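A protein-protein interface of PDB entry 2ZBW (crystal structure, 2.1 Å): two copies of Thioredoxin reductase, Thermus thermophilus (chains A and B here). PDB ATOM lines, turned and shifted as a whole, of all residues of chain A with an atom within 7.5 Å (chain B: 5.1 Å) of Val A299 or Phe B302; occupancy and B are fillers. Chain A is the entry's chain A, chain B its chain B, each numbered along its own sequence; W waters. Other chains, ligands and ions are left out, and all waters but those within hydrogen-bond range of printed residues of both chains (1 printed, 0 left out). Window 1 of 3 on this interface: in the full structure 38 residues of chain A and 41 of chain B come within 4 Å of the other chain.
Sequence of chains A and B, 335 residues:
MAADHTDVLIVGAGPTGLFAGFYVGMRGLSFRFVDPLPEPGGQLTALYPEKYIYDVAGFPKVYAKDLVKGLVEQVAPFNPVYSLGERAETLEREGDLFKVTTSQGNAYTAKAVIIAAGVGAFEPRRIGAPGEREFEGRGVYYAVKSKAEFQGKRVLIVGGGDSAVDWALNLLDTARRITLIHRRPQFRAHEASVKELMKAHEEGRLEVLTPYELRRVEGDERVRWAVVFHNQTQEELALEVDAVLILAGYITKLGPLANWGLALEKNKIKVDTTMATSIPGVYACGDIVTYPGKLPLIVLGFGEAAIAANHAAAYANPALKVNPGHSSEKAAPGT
Of the 16 printed residues of chain B, 8 touch a printed residue of chain A. Hydrophobic or aromatic side chains of chain B that line the printed part of chain A: Phe B19, Tyr B23, Leu B71, Val B299, Leu B300, Phe B302 and Ala B306. Of the 18 printed residues of chain A, 8 touch a printed residue of chain B. Hydrophobic or aromatic side chains of chain A that line the printed part of chain B: Ala A57, Leu A297, Val A299, Leu A300 and Phe A302. Along chain A the printed residues that touch a printed residue of chain B span positions 55 to 303. Among the printed residues, 14 pairs touch across the chains.
Phe B19 touches Asp A55. Gly A58 touches Leu B71. Val A299 touches Phe B19 (CG2 to CE2, 3.6 Å). Val A299 touches Phe B302 (CG2 to CB, 3.7 Å). Gly B303 touches Val A299. CG1 of Val A299 touches CB of Ala B306 (3.7 Å). Leu A300 touches Gly B303. Val B299 touches Phe A302. Gly A303 touches Val B299. Leu B300 touches Gly A303 (CD1 to O, 3.5 Å).
OD1 of Asp A55 sits at hydrogen-bond distance from OH of Tyr B23, 2.6 Å away.
Printed residues of chain B within 4 Å of Val A299: Phe B19 (3.6 Å), Phe B302 (3.7 Å), Gly B303 (3.8 Å) and Ala B306 (3.7 Å). Phe B302 touches just these residues of chain A: Ala A57 and Val A299. No residue of chain A comes within 4 Å of Gly B301. Of the printed residues of chain A, Ala B306 touches Val A299 (3.7 Å). Printed residues of chain A within 4 Å of Leu B300: Gly A303 (3.5 Å). Of the printed residues of chain B, Asp A55 touches Phe B19 (3.4 Å) and Tyr B23 (2.6 Å). The nearest residue of chain B that does not touch Val A299 is Val B299 (4.5 Å). The nearest residue of chain A that does not touch Phe B302 is Gly A58 (5.2 Å). The nearest printed residue of chain A that does not touch Leu B300 is Glu A304 (4.8 Å).
Water W1 lies within hydrogen-bond range of the backbone carbonyl oxygen of Val B299 and the backbone carbonyl oxygen of Val A299.
Val A299 touches Phe B302, and with the chains exchanged Phe A302 touches Val B299. Val A299 touches Gly B303, and with the chains exchanged Gly A303 touches Val B299. Leu A300 touches Gly B303, and with the chains exchanged Gly A303 touches Leu B300.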
ATOM      1  N   THR A  16     -10.012 -21.785 -28.379  1.00  0.00           N
ATOM      2  CA  THR A  16     -11.310 -22.333 -27.985  1.00  0.00           C
ATOM      3  C   THR A  16     -11.285 -23.867 -27.998  1.00  0.00           C
ATOM      4  O   THR A  16     -11.881 -24.499 -27.133  1.00  0.00           O
ATOM      5  CB  THR A  16     -12.497 -21.787 -28.868  1.00  0.00           C
ATOM      6  OG1 THR A  16     -12.545 -22.467 -30.124  1.00  0.00           O
ATOM      7  CG2 THR A  16     -12.332 -20.291 -29.123  1.00  0.00           C
ATOM      8  N   ILE A  53      -2.328  -9.126 -25.877  1.00  0.00           N
ATOM      9  CA  ILE A  53      -3.780  -9.176 -26.001  1.00  0.00           C
ATOM     10  C   ILE A  53      -4.253  -8.472 -24.733  1.00  0.00           C
ATOM     11  O   ILE A  53      -3.702  -8.714 -23.660  1.00  0.00           O
ATOM     12  CB  ILE A  53      -4.296 -10.627 -26.011  1.00  0.00           C
ATOM     13  CG1 ILE A  53      -3.776 -11.364 -27.252  1.00  0.00           C
ATOM     14  CG2 ILE A  53      -5.807 -10.627 -25.975  1.00  0.00           C
ATOM     15  CD1 ILE A  53      -4.041 -12.872 -27.232  1.00  0.00           C
ATOM     16  N   ASP A  55      -7.941  -7.883 -24.084  1.00  0.00           N
ATOM     17  CA  ASP A  55      -9.324  -8.179 -23.699  1.00  0.00           C
ATOM     18  C   ASP A  55      -9.639  -9.631 -23.337  1.00  0.00           C
ATOM     19  O   ASP A  55     -10.739 -10.119 -23.623  1.00  0.00           O
ATOM     20  CB  ASP A  55     -10.301  -7.710 -24.787  1.00  0.00           C
ATOM     21  CG  ASP A  55     -10.121  -8.463 -26.072  1.00  0.00           C
ATOM     22  OD1 ASP A  55     -10.922  -8.301 -27.015  1.00  0.00           O
ATOM     23  OD2 ASP A  55      -9.153  -9.239 -26.119  1.00  0.00           O
ATOM     24  N   VAL A  56      -8.673 -10.327 -22.743  1.00  0.00           N
ATOM     25  CA  VAL A  56      -8.921 -11.689 -22.281  1.00  0.00           C
ATOM     26  C   VAL A  56      -9.147 -11.480 -20.789  1.00  0.00           C
ATOM     27  O   VAL A  56      -8.273 -10.975 -20.081  1.00  0.00           O
ATOM     28  CB  VAL A  56      -7.725 -12.626 -22.523  1.00  0.00           C
ATOM     29  CG1 VAL A  56      -7.968 -13.984 -21.843  1.00  0.00           C
ATOM     30  CG2 VAL A  56      -7.542 -12.837 -24.021  1.00  0.00           C
ATOM     31  N   ALA A  57     -10.338 -11.834 -20.324  1.00  0.00           N
ATOM     32  CA  ALA A  57     -10.709 -11.630 -18.926  1.00  0.00           C
ATOM     33  C   ALA A  57      -9.679 -12.082 -17.901  1.00  0.00           C
ATOM     34  O   ALA A  57      -9.248 -13.232 -17.907  1.00  0.00           O
ATOM     35  CB  ALA A  57     -12.046 -12.308 -18.646  1.00  0.00           C
ATOM     36  N   GLY A  58      -9.308 -11.166 -17.009  1.00  0.00           N
ATOM     37  CA  GLY A  58      -8.346 -11.480 -15.966  1.00  0.00           C
ATOM     38  C   GLY A  58      -6.904 -11.157 -16.319  1.00  0.00           C
ATOM     39  O   GLY A  58      -6.018 -11.241 -15.475  1.00  0.00           O
ATOM     40  N   LEU A  67      -0.680 -16.895 -23.599  1.00  0.00           N
ATOM     41  CA  LEU A  67      -2.039 -17.343 -23.311  1.00  0.00           C
ATOM     42  C   LEU A  67      -2.139 -18.782 -23.796  1.00  0.00           C
ATOM     43  O   LEU A  67      -2.744 -19.630 -23.137  1.00  0.00           O
ATOM     44  CB  LEU A  67      -3.081 -16.478 -24.035  1.00  0.00           C
ATOM     45  CG  LEU A  67      -4.549 -16.908 -23.869  1.00  0.00           C
ATOM     46  CD1 LEU A  67      -4.932 -16.910 -22.401  1.00  0.00           C
ATOM     47  CD2 LEU A  67      -5.465 -15.974 -24.652  1.00  0.00           C
ATOM     48  N   LEU A 295     -19.404 -12.418 -31.667  1.00  0.00           N
ATOM     49  CA  LEU A 295     -18.287 -11.514 -31.884  1.00  0.00           C
ATOM     50  C   LEU A 295     -17.030 -12.375 -31.978  1.00  0.00           C
ATOM     51  O   LEU A 295     -16.877 -13.343 -31.231  1.00  0.00           O
ATOM     52  CB  LEU A 295     -18.163 -10.520 -30.724  1.00  0.00           C
ATOM     53  CG  LEU A 295     -19.355  -9.578 -30.534  1.00  0.00           C
ATOM     54  CD1 LEU A 295     -19.119  -8.662 -29.346  1.00  0.00           C
ATOM     55  CD2 LEU A 295     -19.559  -8.765 -31.813  1.00  0.00           C
ATOM     56  N   PRO A 296     -16.128 -12.046 -32.915  1.00  0.00           N
ATOM     57  CA  PRO A 296     -14.880 -12.797 -33.105  1.00  0.00           C
ATOM     58  C   PRO A 296     -13.868 -12.458 -32.015  1.00  0.00           C
ATOM     59  O   PRO A 296     -12.802 -11.896 -32.301  1.00  0.00           O
ATOM     60  CB  PRO A 296     -14.414 -12.335 -34.481  1.00  0.00           C
ATOM     61  CG  PRO A 296     -14.808 -10.889 -34.467  1.00  0.00           C
ATOM     62  CD  PRO A 296     -16.227 -10.947 -33.892  1.00  0.00           C
ATOM     63  N   LEU A 297     -14.211 -12.802 -30.770  1.00  0.00           N
ATOM     64  CA  LEU A 297     -13.351 -12.540 -29.622  1.00  0.00           C
ATOM     65  C   LEU A 297     -12.963 -13.827 -28.920  1.00  0.00           C
ATOM     66  O   LEU A 297     -13.735 -14.786 -28.864  1.00  0.00           O
ATOM     67  CB  LEU A 297     -14.061 -11.635 -28.611  1.00  0.00           C
ATOM     68  CG  LEU A 297     -14.630 -10.300 -29.110  1.00  0.00           C
ATOM     69  CD1 LEU A 297     -15.538  -9.691 -28.042  1.00  0.00           C
ATOM     70  CD2 LEU A 297     -13.492  -9.360 -29.459  1.00  0.00           C
ATOM     71  N   ILE A 298     -11.754 -13.833 -28.384  1.00  0.00           N
ATOM     72  CA  ILE A 298     -11.241 -14.969 -27.648  1.00  0.00           C
ATOM     73  C   ILE A 298     -12.106 -15.224 -26.407  1.00  0.00           C
ATOM     74  O   ILE A 298     -12.544 -16.341 -26.165  1.00  0.00           O
ATOM     75  CB  ILE A 298      -9.804 -14.696 -27.180  1.00  0.00           C
ATOM     76  CG1 ILE A 298      -8.876 -14.577 -28.387  1.00  0.00           C
ATOM     77  CG2 ILE A 298      -9.350 -15.784 -26.214  1.00  0.00           C
ATOM     78  CD1 ILE A 298      -7.490 -14.057 -28.011  1.00  0.00           C
ATOM     79  N   VAL A 299     -12.354 -14.175 -25.629  1.00  0.00           N
ATOM     80  CA  VAL A 299     -13.131 -14.318 -24.406  1.00  0.00           C
ATOM     81  C   VAL A 299     -14.484 -14.987 -24.640  1.00  0.00           C
ATOM     82  O   VAL A 299     -14.931 -15.787 -23.821  1.00  0.00           O
ATOM     83  CB  VAL A 299     -13.336 -12.951 -23.696  1.00  0.00           C
ATOM     84  CG1 VAL A 299     -14.109 -11.993 -24.600  1.00  0.00           C
ATOM     85  CG2 VAL A 299     -14.075 -13.159 -22.374  1.00  0.00           C
ATOM     86  N   LEU A 300     -15.129 -14.665 -25.757  1.00  0.00           N
ATOM     87  CA  LEU A 300     -16.428 -15.247 -26.066  1.00  0.00           C
ATOM     88  C   LEU A 300     -16.241 -16.695 -26.508  1.00  0.00           C
ATOM     89  O   LEU A 300     -17.066 -17.568 -26.209  1.00  0.00           O
ATOM     90  CB  LEU A 300     -17.119 -14.438 -27.169  1.00  0.00           C
ATOM     91  CG  LEU A 300     -18.505 -14.912 -27.606  1.00  0.00           C
ATOM     92  CD1 LEU A 300     -19.371 -15.143 -26.383  1.00  0.00           C
ATOM     93  CD2 LEU A 300     -19.144 -13.872 -28.521  1.00  0.00           C
ATOM     94  N   GLY A 301     -15.149 -16.941 -27.226  1.00  0.00           N
ATOM     95  CA  GLY A 301     -14.856 -18.287 -27.684  1.00  0.00           C
ATOM     96  C   GLY A 301     -14.698 -19.238 -26.507  1.00  0.00           C
ATOM     97  O   GLY A 301     -15.107 -20.394 -26.586  1.00  0.00           O
ATOM     98  N   PHE A 302     -14.104 -18.763 -25.413  1.00  0.00           N
ATOM     99  CA  PHE A 302     -13.923 -19.614 -24.240  1.00  0.00           C
ATOM    100  C   PHE A 302     -15.290 -19.991 -23.654  1.00  0.00           C
ATOM    101  O   PHE A 302     -15.504 -21.132 -23.232  1.00  0.00           O
ATOM    102  CB  PHE A 302     -13.088 -18.910 -23.159  1.00  0.00           C
ATOM    103  CG  PHE A 302     -11.621 -18.737 -23.509  1.00  0.00           C
ATOM    104  CD1 PHE A 302     -10.923 -19.734 -24.187  1.00  0.00           C
ATOM    105  CD2 PHE A 302     -10.927 -17.604 -23.086  1.00  0.00           C
ATOM    106  CE1 PHE A 302      -9.556 -19.608 -24.434  1.00  0.00           C
ATOM    107  CE2 PHE A 302      -9.551 -17.467 -23.327  1.00  0.00           C
ATOM    108  CZ  PHE A 302      -8.866 -18.466 -23.999  1.00  0.00           C
ATOM    109  N   GLY A 303     -16.205 -19.023 -23.631  1.00  0.00           N
ATOM    110  CA  GLY A 303     -17.532 -19.259 -23.094  1.00  0.00           C
ATOM    111  C   GLY A 303     -18.286 -20.271 -23.925  1.00  0.00           C
ATOM    112  O   GLY A 303     -18.965 -21.152 -23.391  1.00  0.00           O
ATOM    113  N   GLU A 304     -18.157 -20.144 -25.242  1.00  0.00           N
ATOM    114  CA  GLU A 304     -18.805 -21.050 -26.175  1.00  0.00           C
ATOM    115  C   GLU A 304     -18.211 -22.449 -26.048  1.00  0.00           C
ATOM    116  O   GLU A 304     -18.923 -23.444 -26.188  1.00  0.00           O
ATOM    117  CB  GLU A 304     -18.630 -20.531 -27.600  1.00  0.00           C
ATOM    118  CG  GLU A 304     -19.350 -19.207 -27.877  1.00  0.00           C
ATOM    119  CD  GLU A 304     -18.857 -18.549 -29.147  1.00  0.00           C
ATOM    120  OE1 GLU A 304     -19.477 -17.559 -29.599  1.00  0.00           O
ATOM    121  OE2 GLU A 304     -17.841 -19.027 -29.690  1.00  0.00           O
ATOM    122  N   ALA A 305     -16.901 -22.514 -25.794  1.00  0.00           N
ATOM    123  CA  ALA A 305     -16.202 -23.789 -25.637  1.00  0.00           C
ATOM    124  C   ALA A 305     -16.657 -24.511 -24.364  1.00  0.00           C
ATOM    125  O   ALA A 305     -16.748 -25.733 -24.343  1.00  0.00           O
ATOM    126  CB  ALA A 305     -14.684 -23.568 -25.595  1.00  0.00           C
ATOM    127  N   PRO B  15     -17.482 -10.622 -10.988  1.00  0.00           N
ATOM    128  CA  PRO B  15     -16.610 -10.796 -12.153  1.00  0.00           C
ATOM    129  C   PRO B  15     -17.194 -10.425 -13.524  1.00  0.00           C
ATOM    130  O   PRO B  15     -16.498  -9.802 -14.330  1.00  0.00           O
ATOM    131  CB  PRO B  15     -16.191 -12.264 -12.067  1.00  0.00           C
ATOM    132  CG  PRO B  15     -17.313 -12.906 -11.314  1.00  0.00           C
ATOM    133  CD  PRO B  15     -17.647 -11.888 -10.255  1.00  0.00           C
ATOM    134  N   THR B  16     -18.451 -10.780 -13.801  1.00  0.00           N
ATOM    135  CA  THR B  16     -18.992 -10.436 -15.114  1.00  0.00           C
ATOM    136  C   THR B  16     -19.213  -8.922 -15.236  1.00  0.00           C
ATOM    137  O   THR B  16     -18.930  -8.331 -16.273  1.00  0.00           O
ATOM    138  CB  THR B  16     -20.321 -11.194 -15.437  1.00  0.00           C
ATOM    139  OG1 THR B  16     -21.396 -10.660 -14.660  1.00  0.00           O
ATOM    140  CG2 THR B  16     -20.175 -12.679 -15.130  1.00  0.00           C
ATOM    141  N   PHE B  19     -15.849  -7.196 -15.897  1.00  0.00           N
ATOM    142  CA  PHE B  19     -15.366  -7.342 -17.265  1.00  0.00           C
ATOM    143  C   PHE B  19     -16.222  -6.546 -18.244  1.00  0.00           C
ATOM    144  O   PHE B  19     -15.715  -6.033 -19.242  1.00  0.00           O
ATOM    145  CB  PHE B  19     -15.335  -8.806 -17.691  1.00  0.00           C
ATOM    146  CG  PHE B  19     -14.549  -9.041 -18.941  1.00  0.00           C
ATOM    147  CD1 PHE B  19     -13.200  -8.706 -18.998  1.00  0.00           C
ATOM    148  CD2 PHE B  19     -15.156  -9.560 -20.077  1.00  0.00           C
ATOM    149  CE1 PHE B  19     -12.465  -8.882 -20.170  1.00  0.00           C
ATOM    150  CE2 PHE B  19     -14.431  -9.742 -21.250  1.00  0.00           C
ATOM    151  CZ  PHE B  19     -13.079  -9.400 -21.297  1.00  0.00           C
ATOM    152  N   TYR B  23     -15.013  -3.651 -20.909  1.00  0.00           N
ATOM    153  CA  TYR B  23     -15.295  -3.485 -22.330  1.00  0.00           C
ATOM    154  C   TYR B  23     -16.019  -2.197 -22.659  1.00  0.00           C
ATOM    155  O   TYR B  23     -15.768  -1.601 -23.709  1.00  0.00           O
ATOM    156  CB  TYR B  23     -16.035  -4.693 -22.915  1.00  0.00           C
ATOM    157  CG  TYR B  23     -15.270  -5.239 -24.102  1.00  0.00           C
ATOM    158  CD1 TYR B  23     -15.019  -4.431 -25.217  1.00  0.00           C
ATOM    159  CD2 TYR B  23     -14.683  -6.506 -24.065  1.00  0.00           C
ATOM    160  CE1 TYR B  23     -14.192  -4.865 -26.259  1.00  0.00           C
ATOM    161  CE2 TYR B  23     -13.848  -6.949 -25.110  1.00  0.00           C
ATOM    162  CZ  TYR B  23     -13.606  -6.121 -26.198  1.00  0.00           C
ATOM    163  OH  TYR B  23     -12.759  -6.526 -27.209  1.00  0.00           O
ATOM    164  N   VAL B  56     -11.196 -21.191 -15.193  1.00  0.00           N
ATOM    165  CA  VAL B  56     -11.219 -19.873 -15.833  1.00  0.00           C
ATOM    166  C   VAL B  56     -10.133 -19.994 -16.907  1.00  0.00           C
ATOM    167  O   VAL B  56      -8.978 -20.316 -16.606  1.00  0.00           O
ATOM    168  CB  VAL B  56     -10.870 -18.743 -14.838  1.00  0.00           C
ATOM    169  CG1 VAL B  56     -10.717 -17.410 -15.572  1.00  0.00           C
ATOM    170  CG2 VAL B  56     -11.967 -18.635 -13.797  1.00  0.00           C
ATOM    171  N   LEU B  67      -8.168 -13.297  -8.887  1.00  0.00           N
ATOM    172  CA  LEU B  67      -8.872 -13.089 -10.153  1.00  0.00           C
ATOM    173  C   LEU B  67      -9.573 -11.738 -10.075  1.00  0.00           C
ATOM    174  O   LEU B  67      -9.580 -10.973 -11.040  1.00  0.00           O
ATOM    175  CB  LEU B  67      -9.897 -14.202 -10.414  1.00  0.00           C
ATOM    176  CG  LEU B  67     -10.751 -14.053 -11.681  1.00  0.00           C
ATOM    177  CD1 LEU B  67      -9.854 -13.929 -12.913  1.00  0.00           C
ATOM    178  CD2 LEU B  67     -11.676 -15.250 -11.816  1.00  0.00           C
ATOM    179  N   LEU B  71      -9.087  -8.481 -12.514  1.00  0.00           N
ATOM    180  CA  LEU B  71     -10.173  -7.799 -13.204  1.00  0.00           C
ATOM    181  C   LEU B  71     -10.226  -6.318 -12.821  1.00  0.00           C
ATOM    182  O   LEU B  71     -10.456  -5.457 -13.671  1.00  0.00           O
ATOM    183  CB  LEU B  71     -11.508  -8.478 -12.878  1.00  0.00           C
ATOM    184  CG  LEU B  71     -11.663  -9.896 -13.447  1.00  0.00           C
ATOM    185  CD1 LEU B  71     -12.859 -10.590 -12.805  1.00  0.00           C
ATOM    186  CD2 LEU B  71     -11.833  -9.816 -14.971  1.00  0.00           C
ATOM    187  N   ILE B 298     -17.962 -18.854 -14.403  1.00  0.00           N
ATOM    188  CA  ILE B 298     -17.245 -17.607 -14.611  1.00  0.00           C
ATOM    189  C   ILE B 298     -16.840 -17.446 -16.081  1.00  0.00           C
ATOM    190  O   ILE B 298     -17.010 -16.370 -16.664  1.00  0.00           O
ATOM    191  CB  ILE B 298     -15.969 -17.552 -13.741  1.00  0.00           C
ATOM    192  CG1 ILE B 298     -16.346 -17.552 -12.252  1.00  0.00           C
ATOM    193  CG2 ILE B 298     -15.160 -16.308 -14.079  1.00  0.00           C
ATOM    194  CD1 ILE B 298     -15.160 -17.710 -11.305  1.00  0.00           C
ATOM    195  N   VAL B 299     -16.327 -18.519 -16.684  1.00  0.00           N
ATOM    196  CA  VAL B 299     -15.874 -18.461 -18.073  1.00  0.00           C
ATOM    197  C   VAL B 299     -16.966 -18.068 -19.054  1.00  0.00           C
ATOM    198  O   VAL B 299     -16.713 -17.337 -20.010  1.00  0.00           O
ATOM    199  CB  VAL B 299     -15.212 -19.809 -18.531  1.00  0.00           C
ATOM    200  CG1 VAL B 299     -16.187 -20.961 -18.419  1.00  0.00           C
ATOM    201  CG2 VAL B 299     -14.699 -19.666 -19.970  1.00  0.00           C
ATOM    202  N   LEU B 300     -18.176 -18.551 -18.823  1.00  0.00           N
ATOM    203  CA  LEU B 300     -19.294 -18.217 -19.687  1.00  0.00           C
ATOM    204  C   LEU B 300     -19.752 -16.802 -19.345  1.00  0.00           C
ATOM    205  O   LEU B 300     -20.158 -16.044 -20.226  1.00  0.00           O
ATOM    206  CB  LEU B 300     -20.429 -19.215 -19.472  1.00  0.00           C
ATOM    207  CG  LEU B 300     -21.666 -19.105 -20.353  1.00  0.00           C
ATOM    208  CD1 LEU B 300     -21.258 -18.978 -21.819  1.00  0.00           C
ATOM    209  CD2 LEU B 300     -22.547 -20.333 -20.118  1.00  0.00           C
ATOM    210  N   GLY B 301     -19.678 -16.452 -18.060  1.00  0.00           N
ATOM    211  CA  GLY B 301     -20.070 -15.122 -17.628  1.00  0.00           C
ATOM    212  C   GLY B 301     -19.227 -14.039 -18.296  1.00  0.00           C
ATOM    213  O   GLY B 301     -19.733 -12.971 -18.652  1.00  0.00           O
ATOM    214  N   PHE B 302     -17.938 -14.305 -18.469  1.00  0.00           N
ATOM    215  CA  PHE B 302     -17.059 -13.335 -19.115  1.00  0.00           C
ATOM    216  C   PHE B 302     -17.471 -13.139 -20.572  1.00  0.00           C
ATOM    217  O   PHE B 302     -17.552 -12.009 -21.052  1.00  0.00           O
ATOM    218  CB  PHE B 302     -15.596 -13.789 -19.053  1.00  0.00           C
ATOM    219  CG  PHE B 302     -14.956 -13.626 -17.696  1.00  0.00           C
ATOM    220  CD1 PHE B 302     -15.225 -12.512 -16.911  1.00  0.00           C
ATOM    221  CD2 PHE B 302     -14.038 -14.567 -17.230  1.00  0.00           C
ATOM    222  CE1 PHE B 302     -14.590 -12.333 -15.681  1.00  0.00           C
ATOM    223  CE2 PHE B 302     -13.397 -14.399 -16.009  1.00  0.00           C
ATOM    224  CZ  PHE B 302     -13.674 -13.277 -15.229  1.00  0.00           C
ATOM    225  N   GLY B 303     -17.730 -14.240 -21.274  1.00  0.00           N
ATOM    226  CA  GLY B 303     -18.137 -14.143 -22.664  1.00  0.00           C
ATOM    227  C   GLY B 303     -19.448 -13.389 -22.819  1.00  0.00           C
ATOM    228  O   GLY B 303     -19.642 -12.615 -23.763  1.00  0.00           O
ATOM    229  N   GLU B 304     -20.358 -13.623 -21.883  1.00  0.00           N
ATOM    230  CA  GLU B 304     -21.654 -12.961 -21.904  1.00  0.00           C
ATOM    231  C   GLU B 304     -21.477 -11.465 -21.670  1.00  0.00           C
ATOM    232  O   GLU B 304     -22.198 -10.644 -22.241  1.00  0.00           O
ATOM    233  CB  GLU B 304     -22.553 -13.571 -20.823  1.00  0.00           C
ATOM    234  CG  GLU B 304     -22.986 -15.000 -21.129  1.00  0.00           C
ATOM    235  CD  GLU B 304     -23.687 -15.660 -19.957  1.00  0.00           C
ATOM    236  OE1 GLU B 304     -24.210 -16.777 -20.133  1.00  0.00           O
ATOM    237  OE2 GLU B 304     -23.706 -15.068 -18.855  1.00  0.00           O
ATOM    238  N   ALA B 305     -20.506 -11.117 -20.828  1.00  0.00           N
ATOM    239  CA  ALA B 305     -20.233  -9.723 -20.500  1.00  0.00           C
ATOM    240  C   ALA B 305     -19.682  -9.005 -21.733  1.00  0.00           C
ATOM    241  O   ALA B 305     -20.052  -7.861 -22.014  1.00  0.00           O
ATOM    242  CB  ALA B 305     -19.231  -9.631 -19.328  1.00  0.00           C
ATOM    243  N   ALA B 306     -18.807  -9.686 -22.467  1.00  0.00           N
ATOM    244  CA  ALA B 306     -18.230  -9.101 -23.671  1.00  0.00           C
ATOM    245  C   ALA B 306     -19.352  -8.741 -24.635  1.00  0.00           C
ATOM    246  O   ALA B 306     -19.365  -7.653 -25.211  1.00  0.00           O
ATOM    247  CB  ALA B 306     -17.264 -10.077 -24.326  1.00  0.00           C
HETATM  248  O   HOH W   1     -14.299 -16.428 -21.085  1.00  0.00           O
